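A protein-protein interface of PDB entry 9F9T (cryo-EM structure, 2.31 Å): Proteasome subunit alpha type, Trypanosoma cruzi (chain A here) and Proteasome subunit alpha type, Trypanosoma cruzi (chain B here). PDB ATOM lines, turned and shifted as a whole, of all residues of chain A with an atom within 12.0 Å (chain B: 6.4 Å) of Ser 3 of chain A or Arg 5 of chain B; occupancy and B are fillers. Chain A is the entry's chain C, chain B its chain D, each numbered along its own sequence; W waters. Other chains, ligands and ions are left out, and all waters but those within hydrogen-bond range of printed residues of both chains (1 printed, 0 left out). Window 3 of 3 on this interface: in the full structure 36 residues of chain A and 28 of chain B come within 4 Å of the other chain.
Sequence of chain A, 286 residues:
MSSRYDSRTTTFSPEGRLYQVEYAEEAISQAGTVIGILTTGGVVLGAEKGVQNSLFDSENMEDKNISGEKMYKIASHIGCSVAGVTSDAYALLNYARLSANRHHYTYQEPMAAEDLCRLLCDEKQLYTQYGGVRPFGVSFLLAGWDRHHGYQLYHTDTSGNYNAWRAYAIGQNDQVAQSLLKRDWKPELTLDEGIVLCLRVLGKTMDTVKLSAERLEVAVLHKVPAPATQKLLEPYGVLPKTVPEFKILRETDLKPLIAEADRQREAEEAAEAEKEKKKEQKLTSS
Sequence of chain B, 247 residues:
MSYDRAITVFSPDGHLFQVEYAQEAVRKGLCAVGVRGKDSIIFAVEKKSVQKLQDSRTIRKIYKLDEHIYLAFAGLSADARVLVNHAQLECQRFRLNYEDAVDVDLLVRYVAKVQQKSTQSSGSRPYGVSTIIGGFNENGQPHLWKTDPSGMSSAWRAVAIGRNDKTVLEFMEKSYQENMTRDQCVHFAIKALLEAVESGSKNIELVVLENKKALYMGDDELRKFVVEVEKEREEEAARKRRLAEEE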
ATOM      1  N   SER A   2      30.703  33.334 -29.942  1.00  0.00           N
ATOM      2  CA  SER A   2      30.691  31.922 -29.461  1.00  0.00           C
ATOM      3  C   SER A   2      29.243  31.430 -29.267  1.00  0.00           C
ATOM      4  O   SER A   2      29.003  30.222 -29.395  1.00  0.00           O
ATOM      5  CB  SER A   2      31.536  31.722 -28.180  1.00  0.00           C
ATOM      6  OG  SER A   2      32.394  30.579 -28.240  1.00  0.00           O
ATOM      7  N   SER A   3      28.280  32.328 -28.963  1.00  0.00           N
ATOM      8  CA  SER A   3      26.885  31.924 -28.783  1.00  0.00           C
ATOM      9  C   SER A   3      26.255  31.356 -30.065  1.00  0.00           C
ATOM     10  O   SER A   3      25.300  30.597 -29.958  1.00  0.00           O
ATOM     11  CB  SER A   3      26.023  33.047 -28.225  1.00  0.00           C
ATOM     12  OG  SER A   3      25.840  34.089 -29.177  1.00  0.00           O
ATOM     13  N   ARG A   4      26.805  31.662 -31.254  1.00  0.00           N
ATOM     14  CA  ARG A   4      26.334  31.087 -32.509  1.00  0.00           C
ATOM     15  C   ARG A   4      26.736  29.617 -32.677  1.00  0.00           C
ATOM     16  O   ARG A   4      26.170  28.935 -33.527  1.00  0.00           O
ATOM     17  CB  ARG A   4      26.765  31.936 -33.718  1.00  0.00           C
ATOM     18  CG  ARG A   4      28.246  31.900 -34.060  1.00  0.00           C
ATOM     19  CD  ARG A   4      28.702  33.039 -34.964  1.00  0.00           C
ATOM     20  NE  ARG A   4      28.422  32.793 -36.377  1.00  0.00           N
ATOM     21  CZ  ARG A   4      27.945  33.696 -37.231  1.00  0.00           C
ATOM     22  NH1 ARG A   4      27.716  33.350 -38.486  1.00  0.00           N
ATOM     23  NH2 ARG A   4      27.701  34.937 -36.838  1.00  0.00           N
ATOM     24  N   TYR A   5      27.691  29.119 -31.876  1.00  0.00           N
ATOM     25  CA  TYR A   5      28.170  27.738 -31.942  1.00  0.00           C
ATOM     26  C   TYR A   5      27.561  26.907 -30.808  1.00  0.00           C
ATOM     27  O   TYR A   5      27.967  25.764 -30.613  1.00  0.00           O
ATOM     28  CB  TYR A   5      29.714  27.715 -31.907  1.00  0.00           C
ATOM     29  CG  TYR A   5      30.427  28.605 -32.940  1.00  0.00           C
ATOM     30  CD1 TYR A   5      30.219  28.446 -34.311  1.00  0.00           C
ATOM     31  CD2 TYR A   5      31.248  29.674 -32.533  1.00  0.00           C
ATOM     32  CE1 TYR A   5      30.850  29.271 -35.240  1.00  0.00           C
ATOM     33  CE2 TYR A   5      31.858  30.524 -33.449  1.00  0.00           C
ATOM     34  CZ  TYR A   5      31.673  30.309 -34.809  1.00  0.00           C
ATOM     35  OH  TYR A   5      32.290  31.147 -35.693  1.00  0.00           O
ATOM     36  N   ASP A   6      26.637  27.512 -30.032  1.00  0.00           N
ATOM     37  CA  ASP A   6      25.871  26.853 -28.975  1.00  0.00           C
ATOM     38  C   ASP A   6      24.886  25.917 -29.662  1.00  0.00           C
ATOM     39  O   ASP A   6      24.326  26.278 -30.693  1.00  0.00           O
ATOM     40  CB  ASP A   6      25.184  27.874 -28.043  1.00  0.00           C
ATOM     41  CG  ASP A   6      24.479  27.343 -26.800  1.00  0.00           C
ATOM     42  OD1 ASP A   6      24.323  26.132 -26.713  1.00  0.00           O
ATOM     43  OD2 ASP A   6      24.093  28.161 -25.901  1.00  0.00           O
ATOM     44  N   SER A   7      24.767  24.706 -29.108  1.00  0.00           N
ATOM     45  CA  SER A   7      23.972  23.595 -29.622  1.00  0.00           C
ATOM     46  C   SER A   7      22.534  23.623 -29.083  1.00  0.00           C
ATOM     47  O   SER A   7      21.609  23.120 -29.716  1.00  0.00           O
ATOM     48  CB  SER A   7      24.672  22.305 -29.231  1.00  0.00           C
ATOM     49  OG  SER A   7      25.174  22.376 -27.879  1.00  0.00           O
ATOM     50  N   ARG A   8      22.385  24.157 -27.861  1.00  0.00           N
ATOM     51  CA  ARG A   8      21.110  24.526 -27.274  1.00  0.00           C
ATOM     52  C   ARG A   8      20.440  23.247 -26.751  1.00  0.00           C
ATOM     53  O   ARG A   8      19.284  22.930 -27.066  1.00  0.00           O
ATOM     54  CB  ARG A   8      20.308  25.393 -28.257  1.00  0.00           C
ATOM     55  CG  ARG A   8      20.911  26.780 -28.483  1.00  0.00           C
ATOM     56  CD  ARG A   8      20.134  27.710 -29.410  1.00  0.00           C
ATOM     57  NE  ARG A   8      20.827  28.982 -29.630  1.00  0.00           N
ATOM     58  CZ  ARG A   8      20.905  29.989 -28.750  1.00  0.00           C
ATOM     59  NH1 ARG A   8      21.715  31.011 -28.989  1.00  0.00           N
ATOM     60  NH2 ARG A   8      20.206  29.961 -27.623  1.00  0.00           N
ATOM     61  N   THR A   9      21.188  22.563 -25.869  1.00  0.00           N
ATOM     62  CA  THR A   9      20.900  21.202 -25.436  1.00  0.00           C
ATOM     63  C   THR A   9      19.609  21.162 -24.623  1.00  0.00           C
ATOM     64  O   THR A   9      18.974  20.112 -24.554  1.00  0.00           O
ATOM     65  CB  THR A   9      22.068  20.578 -24.628  1.00  0.00           C
ATOM     66  OG1 THR A   9      22.384  21.399 -23.492  1.00  0.00           O
ATOM     67  CG2 THR A   9      23.294  20.314 -25.485  1.00  0.00           C
ATOM     68  N   THR A  10      19.270  22.284 -23.968  1.00  0.00           N
ATOM     69  CA  THR A  10      18.158  22.312 -23.023  1.00  0.00           C
ATOM     70  C   THR A  10      16.927  23.039 -23.579  1.00  0.00           C
ATOM     71  O   THR A  10      15.980  23.236 -22.835  1.00  0.00           O
ATOM     72  CB  THR A  10      18.611  22.895 -21.674  1.00  0.00           C
ATOM     73  OG1 THR A  10      19.351  24.111 -21.864  1.00  0.00           O
ATOM     74  CG2 THR A  10      19.446  21.913 -20.884  1.00  0.00           C
ATOM     75  N   THR A  11      16.908  23.343 -24.880  1.00  0.00           N
ATOM     76  CA  THR A  11      15.890  24.130 -25.569  1.00  0.00           C
ATOM     77  C   THR A  11      14.877  23.200 -26.245  1.00  0.00           C
ATOM     78  O   THR A  11      15.293  22.481 -27.159  1.00  0.00           O
ATOM     79  CB  THR A  11      16.621  25.036 -26.578  1.00  0.00           C
ATOM     80  OG1 THR A  11      17.174  26.177 -25.914  1.00  0.00           O
ATOM     81  CG2 THR A  11      15.779  25.549 -27.723  1.00  0.00           C
ATOM     82  N   PHE A  12      13.572  23.253 -25.851  1.00  0.00           N
ATOM     83  CA  PHE A  12      12.484  22.587 -26.594  1.00  0.00           C
ATOM     84  C   PHE A  12      12.609  22.901 -28.079  1.00  0.00           C
ATOM     85  O   PHE A  12      13.114  23.962 -28.466  1.00  0.00           O
ATOM     86  CB  PHE A  12      11.040  23.013 -26.261  1.00  0.00           C
ATOM     87  CG  PHE A  12      10.466  22.537 -24.948  1.00  0.00           C
ATOM     88  CD1 PHE A  12      10.110  21.223 -24.755  1.00  0.00           C
ATOM     89  CD2 PHE A  12      10.329  23.399 -23.874  1.00  0.00           C
ATOM     90  CE1 PHE A  12       9.610  20.779 -23.532  1.00  0.00           C
ATOM     91  CE2 PHE A  12       9.891  22.950 -22.632  1.00  0.00           C
ATOM     92  CZ  PHE A  12       9.543  21.630 -22.457  1.00  0.00           C
ATOM     93  N   GLN A 129      16.968  20.325 -18.058  1.00  0.00           N
ATOM     94  CA  GLN A 129      16.363  21.653 -17.957  1.00  0.00           C
ATOM     95  C   GLN A 129      17.424  22.772 -17.884  1.00  0.00           C
ATOM     96  O   GLN A 129      17.403  23.702 -18.690  1.00  0.00           O
ATOM     97  CB  GLN A 129      15.381  21.610 -16.785  1.00  0.00           C
ATOM     98  CG  GLN A 129      14.449  22.822 -16.694  1.00  0.00           C
ATOM     99  CD  GLN A 129      13.323  22.559 -15.725  1.00  0.00           C
ATOM    100  OE1 GLN A 129      13.464  21.748 -14.808  1.00  0.00           O
ATOM    101  NE2 GLN A 129      12.215  23.275 -15.895  1.00  0.00           N
ATOM    102  N   TYR A 130      18.384  22.642 -16.952  1.00  0.00           N
ATOM    103  CA  TYR A 130      19.421  23.632 -16.676  1.00  0.00           C
ATOM    104  C   TYR A 130      20.725  23.170 -17.327  1.00  0.00           C
ATOM    105  O   TYR A 130      20.912  21.966 -17.484  1.00  0.00           O
ATOM    106  CB  TYR A 130      19.616  23.802 -15.149  1.00  0.00           C
ATOM    107  CG  TYR A 130      18.361  24.254 -14.395  1.00  0.00           C
ATOM    108  CD1 TYR A 130      17.318  23.369 -14.107  1.00  0.00           C
ATOM    109  CD2 TYR A 130      18.165  25.595 -14.051  1.00  0.00           C
ATOM    110  CE1 TYR A 130      16.131  23.802 -13.528  1.00  0.00           C
ATOM    111  CE2 TYR A 130      16.993  26.035 -13.445  1.00  0.00           C
ATOM    112  CZ  TYR A 130      15.966  25.137 -13.188  1.00  0.00           C
ATOM    113  OH  TYR A 130      14.811  25.559 -12.575  1.00  0.00           O
ATOM    114  N   GLY A 131      21.589  24.132 -17.736  1.00  0.00           N
ATOM    115  CA  GLY A 131      23.046  23.979 -17.697  1.00  0.00           C
ATOM    116  C   GLY A 131      23.785  23.831 -19.045  1.00  0.00           C
ATOM    117  O   GLY A 131      24.997  23.610 -19.044  1.00  0.00           O
ATOM    118  N   GLY A 132      23.101  23.943 -20.200  1.00  0.00           N
ATOM    119  CA  GLY A 132      23.808  23.997 -21.480  1.00  0.00           C
ATOM    120  C   GLY A 132      24.719  22.802 -21.847  1.00  0.00           C
ATOM    121  O   GLY A 132      25.436  22.863 -22.836  1.00  0.00           O
ATOM    122  N   VAL A 133      24.643  21.670 -21.140  1.00  0.00           N
ATOM    123  CA  VAL A 133      25.450  20.497 -21.475  1.00  0.00           C
ATOM    124  C   VAL A 133      24.560  19.295 -21.814  1.00  0.00           C
ATOM    125  O   VAL A 133      23.392  19.256 -21.404  1.00  0.00           O
ATOM    126  CB  VAL A 133      26.419  20.152 -20.321  1.00  0.00           C
ATOM    127  CG1 VAL A 133      27.501  21.225 -20.116  1.00  0.00           C
ATOM    128  CG2 VAL A 133      25.679  19.839 -19.004  1.00  0.00           C
ATOM    129  N   TYR B   3      25.748  28.676 -17.120  1.00  0.00           N
ATOM    130  CA  TYR B   3      25.135  28.930 -18.414  1.00  0.00           C
ATOM    131  C   TYR B   3      23.948  29.871 -18.212  1.00  0.00           C
ATOM    132  O   TYR B   3      23.122  29.685 -17.328  1.00  0.00           O
ATOM    133  CB  TYR B   3      24.864  27.561 -19.044  1.00  0.00           C
ATOM    134  CG  TYR B   3      24.124  27.552 -20.372  1.00  0.00           C
ATOM    135  CD1 TYR B   3      24.791  27.703 -21.578  1.00  0.00           C
ATOM    136  CD2 TYR B   3      22.741  27.360 -20.410  1.00  0.00           C
ATOM    137  CE1 TYR B   3      24.104  27.603 -22.785  1.00  0.00           C
ATOM    138  CE2 TYR B   3      22.052  27.256 -21.612  1.00  0.00           C
ATOM    139  CZ  TYR B   3      22.737  27.373 -22.799  1.00  0.00           C
ATOM    140  OH  TYR B   3      22.019  27.356 -23.959  1.00  0.00           O
ATOM    141  N   ASP B   4      23.912  30.910 -19.041  1.00  0.00           N
ATOM    142  CA  ASP B   4      23.152  32.112 -18.756  1.00  0.00           C
ATOM    143  C   ASP B   4      22.430  32.538 -20.023  1.00  0.00           C
ATOM    144  O   ASP B   4      21.900  33.642 -20.087  1.00  0.00           O
ATOM    145  CB  ASP B   4      24.094  33.224 -18.254  1.00  0.00           C
ATOM    146  CG  ASP B   4      25.175  33.681 -19.248  1.00  0.00           C
ATOM    147  OD1 ASP B   4      24.834  34.366 -20.263  1.00  0.00           O
ATOM    148  OD2 ASP B   4      26.370  33.368 -19.009  1.00  0.00           O
ATOM    149  N   ARG B   5      22.459  31.690 -21.051  1.00  0.00           N
ATOM    150  CA  ARG B   5      21.906  32.069 -22.332  1.00  0.00           C
ATOM    151  C   ARG B   5      20.437  32.405 -22.086  1.00  0.00           C
ATOM    152  O   ARG B   5      19.786  31.869 -21.177  1.00  0.00           O
ATOM    153  CB  ARG B   5      22.090  30.939 -23.362  1.00  0.00           C
ATOM    154  CG  ARG B   5      21.643  31.231 -24.794  1.00  0.00           C
ATOM    155  CD  ARG B   5      22.796  31.501 -25.754  1.00  0.00           C
ATOM    156  NE  ARG B   5      23.785  32.462 -25.251  1.00  0.00           N
ATOM    157  CZ  ARG B   5      25.072  32.200 -25.000  1.00  0.00           C
ATOM    158  NH1 ARG B   5      25.907  33.195 -24.745  1.00  0.00           N
ATOM    159  NH2 ARG B   5      25.536  30.961 -25.051  1.00  0.00           N
ATOM    160  N   ALA B   6      19.938  33.310 -22.924  1.00  0.00           N
ATOM    161  CA  ALA B   6      18.527  33.609 -22.979  1.00  0.00           C
ATOM    162  C   ALA B   6      17.858  32.562 -23.875  1.00  0.00           C
ATOM    163  O   ALA B   6      18.072  32.549 -25.086  1.00  0.00           O
ATOM    164  CB  ALA B   6      18.362  35.029 -23.488  1.00  0.00           C
ATOM    165  N   ILE B   7      17.027  31.709 -23.263  1.00  0.00           N
ATOM    166  CA  ILE B   7      16.330  30.650 -23.979  1.00  0.00           C
ATOM    167  C   ILE B   7      14.936  31.123 -24.384  1.00  0.00           C
ATOM    168  O   ILE B   7      14.640  31.182 -25.578  1.00  0.00           O
ATOM    169  CB  ILE B   7      16.363  29.355 -23.138  1.00  0.00           C
ATOM    170  CG1 ILE B   7      17.813  28.853 -22.983  1.00  0.00           C
ATOM    171  CG2 ILE B   7      15.448  28.290 -23.735  1.00  0.00           C
ATOM    172  CD1 ILE B   7      18.074  27.963 -21.772  1.00  0.00           C
ATOM    173  N   THR B   8      14.113  31.566 -23.422  1.00  0.00           N
ATOM    174  CA  THR B   8      12.758  31.975 -23.765  1.00  0.00           C
ATOM    175  C   THR B   8      12.733  33.463 -24.178  1.00  0.00           C
ATOM    176  O   THR B   8      12.818  34.327 -23.310  1.00  0.00           O
ATOM    177  CB  THR B   8      11.767  31.700 -22.620  1.00  0.00           C
ATOM    178  OG1 THR B   8      12.022  30.454 -21.968  1.00  0.00           O
ATOM    179  CG2 THR B   8      10.327  31.757 -23.100  1.00  0.00           C
ATOM    180  N   SER B 121      13.747  33.022 -16.779  1.00  0.00           N
ATOM    181  CA  SER B 121      15.052  32.842 -16.157  1.00  0.00           C
ATOM    182  C   SER B 121      16.044  32.276 -17.175  1.00  0.00           C
ATOM    183  O   SER B 121      15.951  31.113 -17.549  1.00  0.00           O
ATOM    184  CB  SER B 121      14.971  32.003 -14.873  1.00  0.00           C
ATOM    185  OG  SER B 121      14.695  30.625 -15.130  1.00  0.00           O
ATOM    186  N   SER B 122      16.929  33.163 -17.660  1.00  0.00           N
ATOM    187  CA  SER B 122      18.145  32.829 -18.392  1.00  0.00           C
ATOM    188  C   SER B 122      18.771  31.543 -17.842  1.00  0.00           C
ATOM    189  O   SER B 122      18.829  31.339 -16.616  1.00  0.00           O
ATOM    190  CB  SER B 122      19.174  33.978 -18.307  1.00  0.00           C
ATOM    191  OG  SER B 122      18.794  35.099 -19.108  1.00  0.00           O
ATOM    192  N   GLY B 123      19.261  30.697 -18.766  1.00  0.00           N
ATOM    193  CA  GLY B 123      19.916  29.454 -18.379  1.00  0.00           C
ATOM    194  C   GLY B 123      19.011  28.222 -18.474  1.00  0.00           C
ATOM    195  O   GLY B 123      19.516  27.106 -18.570  1.00  0.00           O
ATOM    196  N   SER B 124      17.684  28.429 -18.518  1.00  0.00           N
ATOM    197  CA  SER B 124      16.713  27.387 -18.246  1.00  0.00           C
ATOM    198  C   SER B 124      15.583  27.459 -19.267  1.00  0.00           C
ATOM    199  O   SER B 124      15.233  28.532 -19.763  1.00  0.00           O
ATOM    200  CB  SER B 124      16.204  27.517 -16.804  1.00  0.00           C
ATOM    201  OG  SER B 124      14.981  26.820 -16.593  1.00  0.00           O
HETATM  202  O   HOH W   1      20.239  25.194 -23.956  1.00  0.00           O
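OD2 of Asp 6 of chain A is in salt-bridge range of NH2 of Arg 5 of chain B (3.3 Å).
The side-chain carboxylate of Asp 6 of chain A lies within hydrogen-bond range of the side-chain hydroxyl of Tyr 3 of chain B.
O of Gly 132 of chain A lies close to OG1 of Thr 9 of chain A (3.4 Å).
OD1 of Asp 6 of chain A is in hydrogen-bond range of N of Arg 8 of chain A (3.0 Å).
O of Arg 5 of chain B is in hydrogen-bond range of N of Gly 123 of chain B.
Among the printed residues, pairs that only touch across the chains: Ser 3 of chain A with Arg 5 of chain B, Arg 8 of chain A with Arg 5 of chain B, Thr 11 of chain A with Ile 7 of chain B, Gln 129 of chain A with Ser 124 of chain B, Tyr 130 of chain A with Gly 123 of chain B, Tyr 130 of chain A with Ser 124 of chain B, Gly 131 of chain A with Tyr 3 of chain B, Gly 131 of chain A with Gly 123 of chain B and Gly 132 of chain A with Tyr 3 of chain B.
Of chain B, only Arg 5 comes within 4 Å of Ser 3 of chain A.
Arg 5 of chain B touches just these residues of chain A: Ser 3 (3.5 Å), Asp 6 (3.3 Å) and Arg 8 (3.4 Å).
No residue of chain A comes within 4 Å of Asp 4 of chain B.
Ala 6 of chain B touches none of the printed residues of chain A.
No residue of chain A comes within 4 Å of Ser 122 of chain B.
Of the printed residues of chain B, Arg 8 of chain A touches Arg 5 (3.4 Å).
Printed residues of chain A within 4 Å of Gly 123 of chain B: Tyr 130 and Gly 131.
Printed residues of chain B within 4 Å of Asp 6 of chain A: Tyr 3 (3.0 Å) and Arg 5 (3.3 Å).
Val 133 of chain A touches none of the printed residues of chain B.
The nearest printed residue of chain B that does not touch Ser 3 of chain A is Tyr 3 of chain B (7.6 Å).
Of the 16 printed residues of chain A, 8 touch a printed residue of chain B.
Printed residues of chain A that touch a printed residue of chain B: Ser 3, Asp 6, Arg 8, Thr 11, Gln 129, Tyr 130, Gly 131 and Gly 132.
Among the printed residues, Asp or Glu carboxylates within 4 Å of a Lys or Arg side-chain nitrogen of the other chain: Asp 6 of chain A with Arg 5 of chain B.
Water W1 lies within hydrogen-bond range of the side-chain hydroxyl of Thr 10 of chain A, the side-chain hydroxyl of Tyr 3 of chain B and the backbone NH of Thr 9 of chain A.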
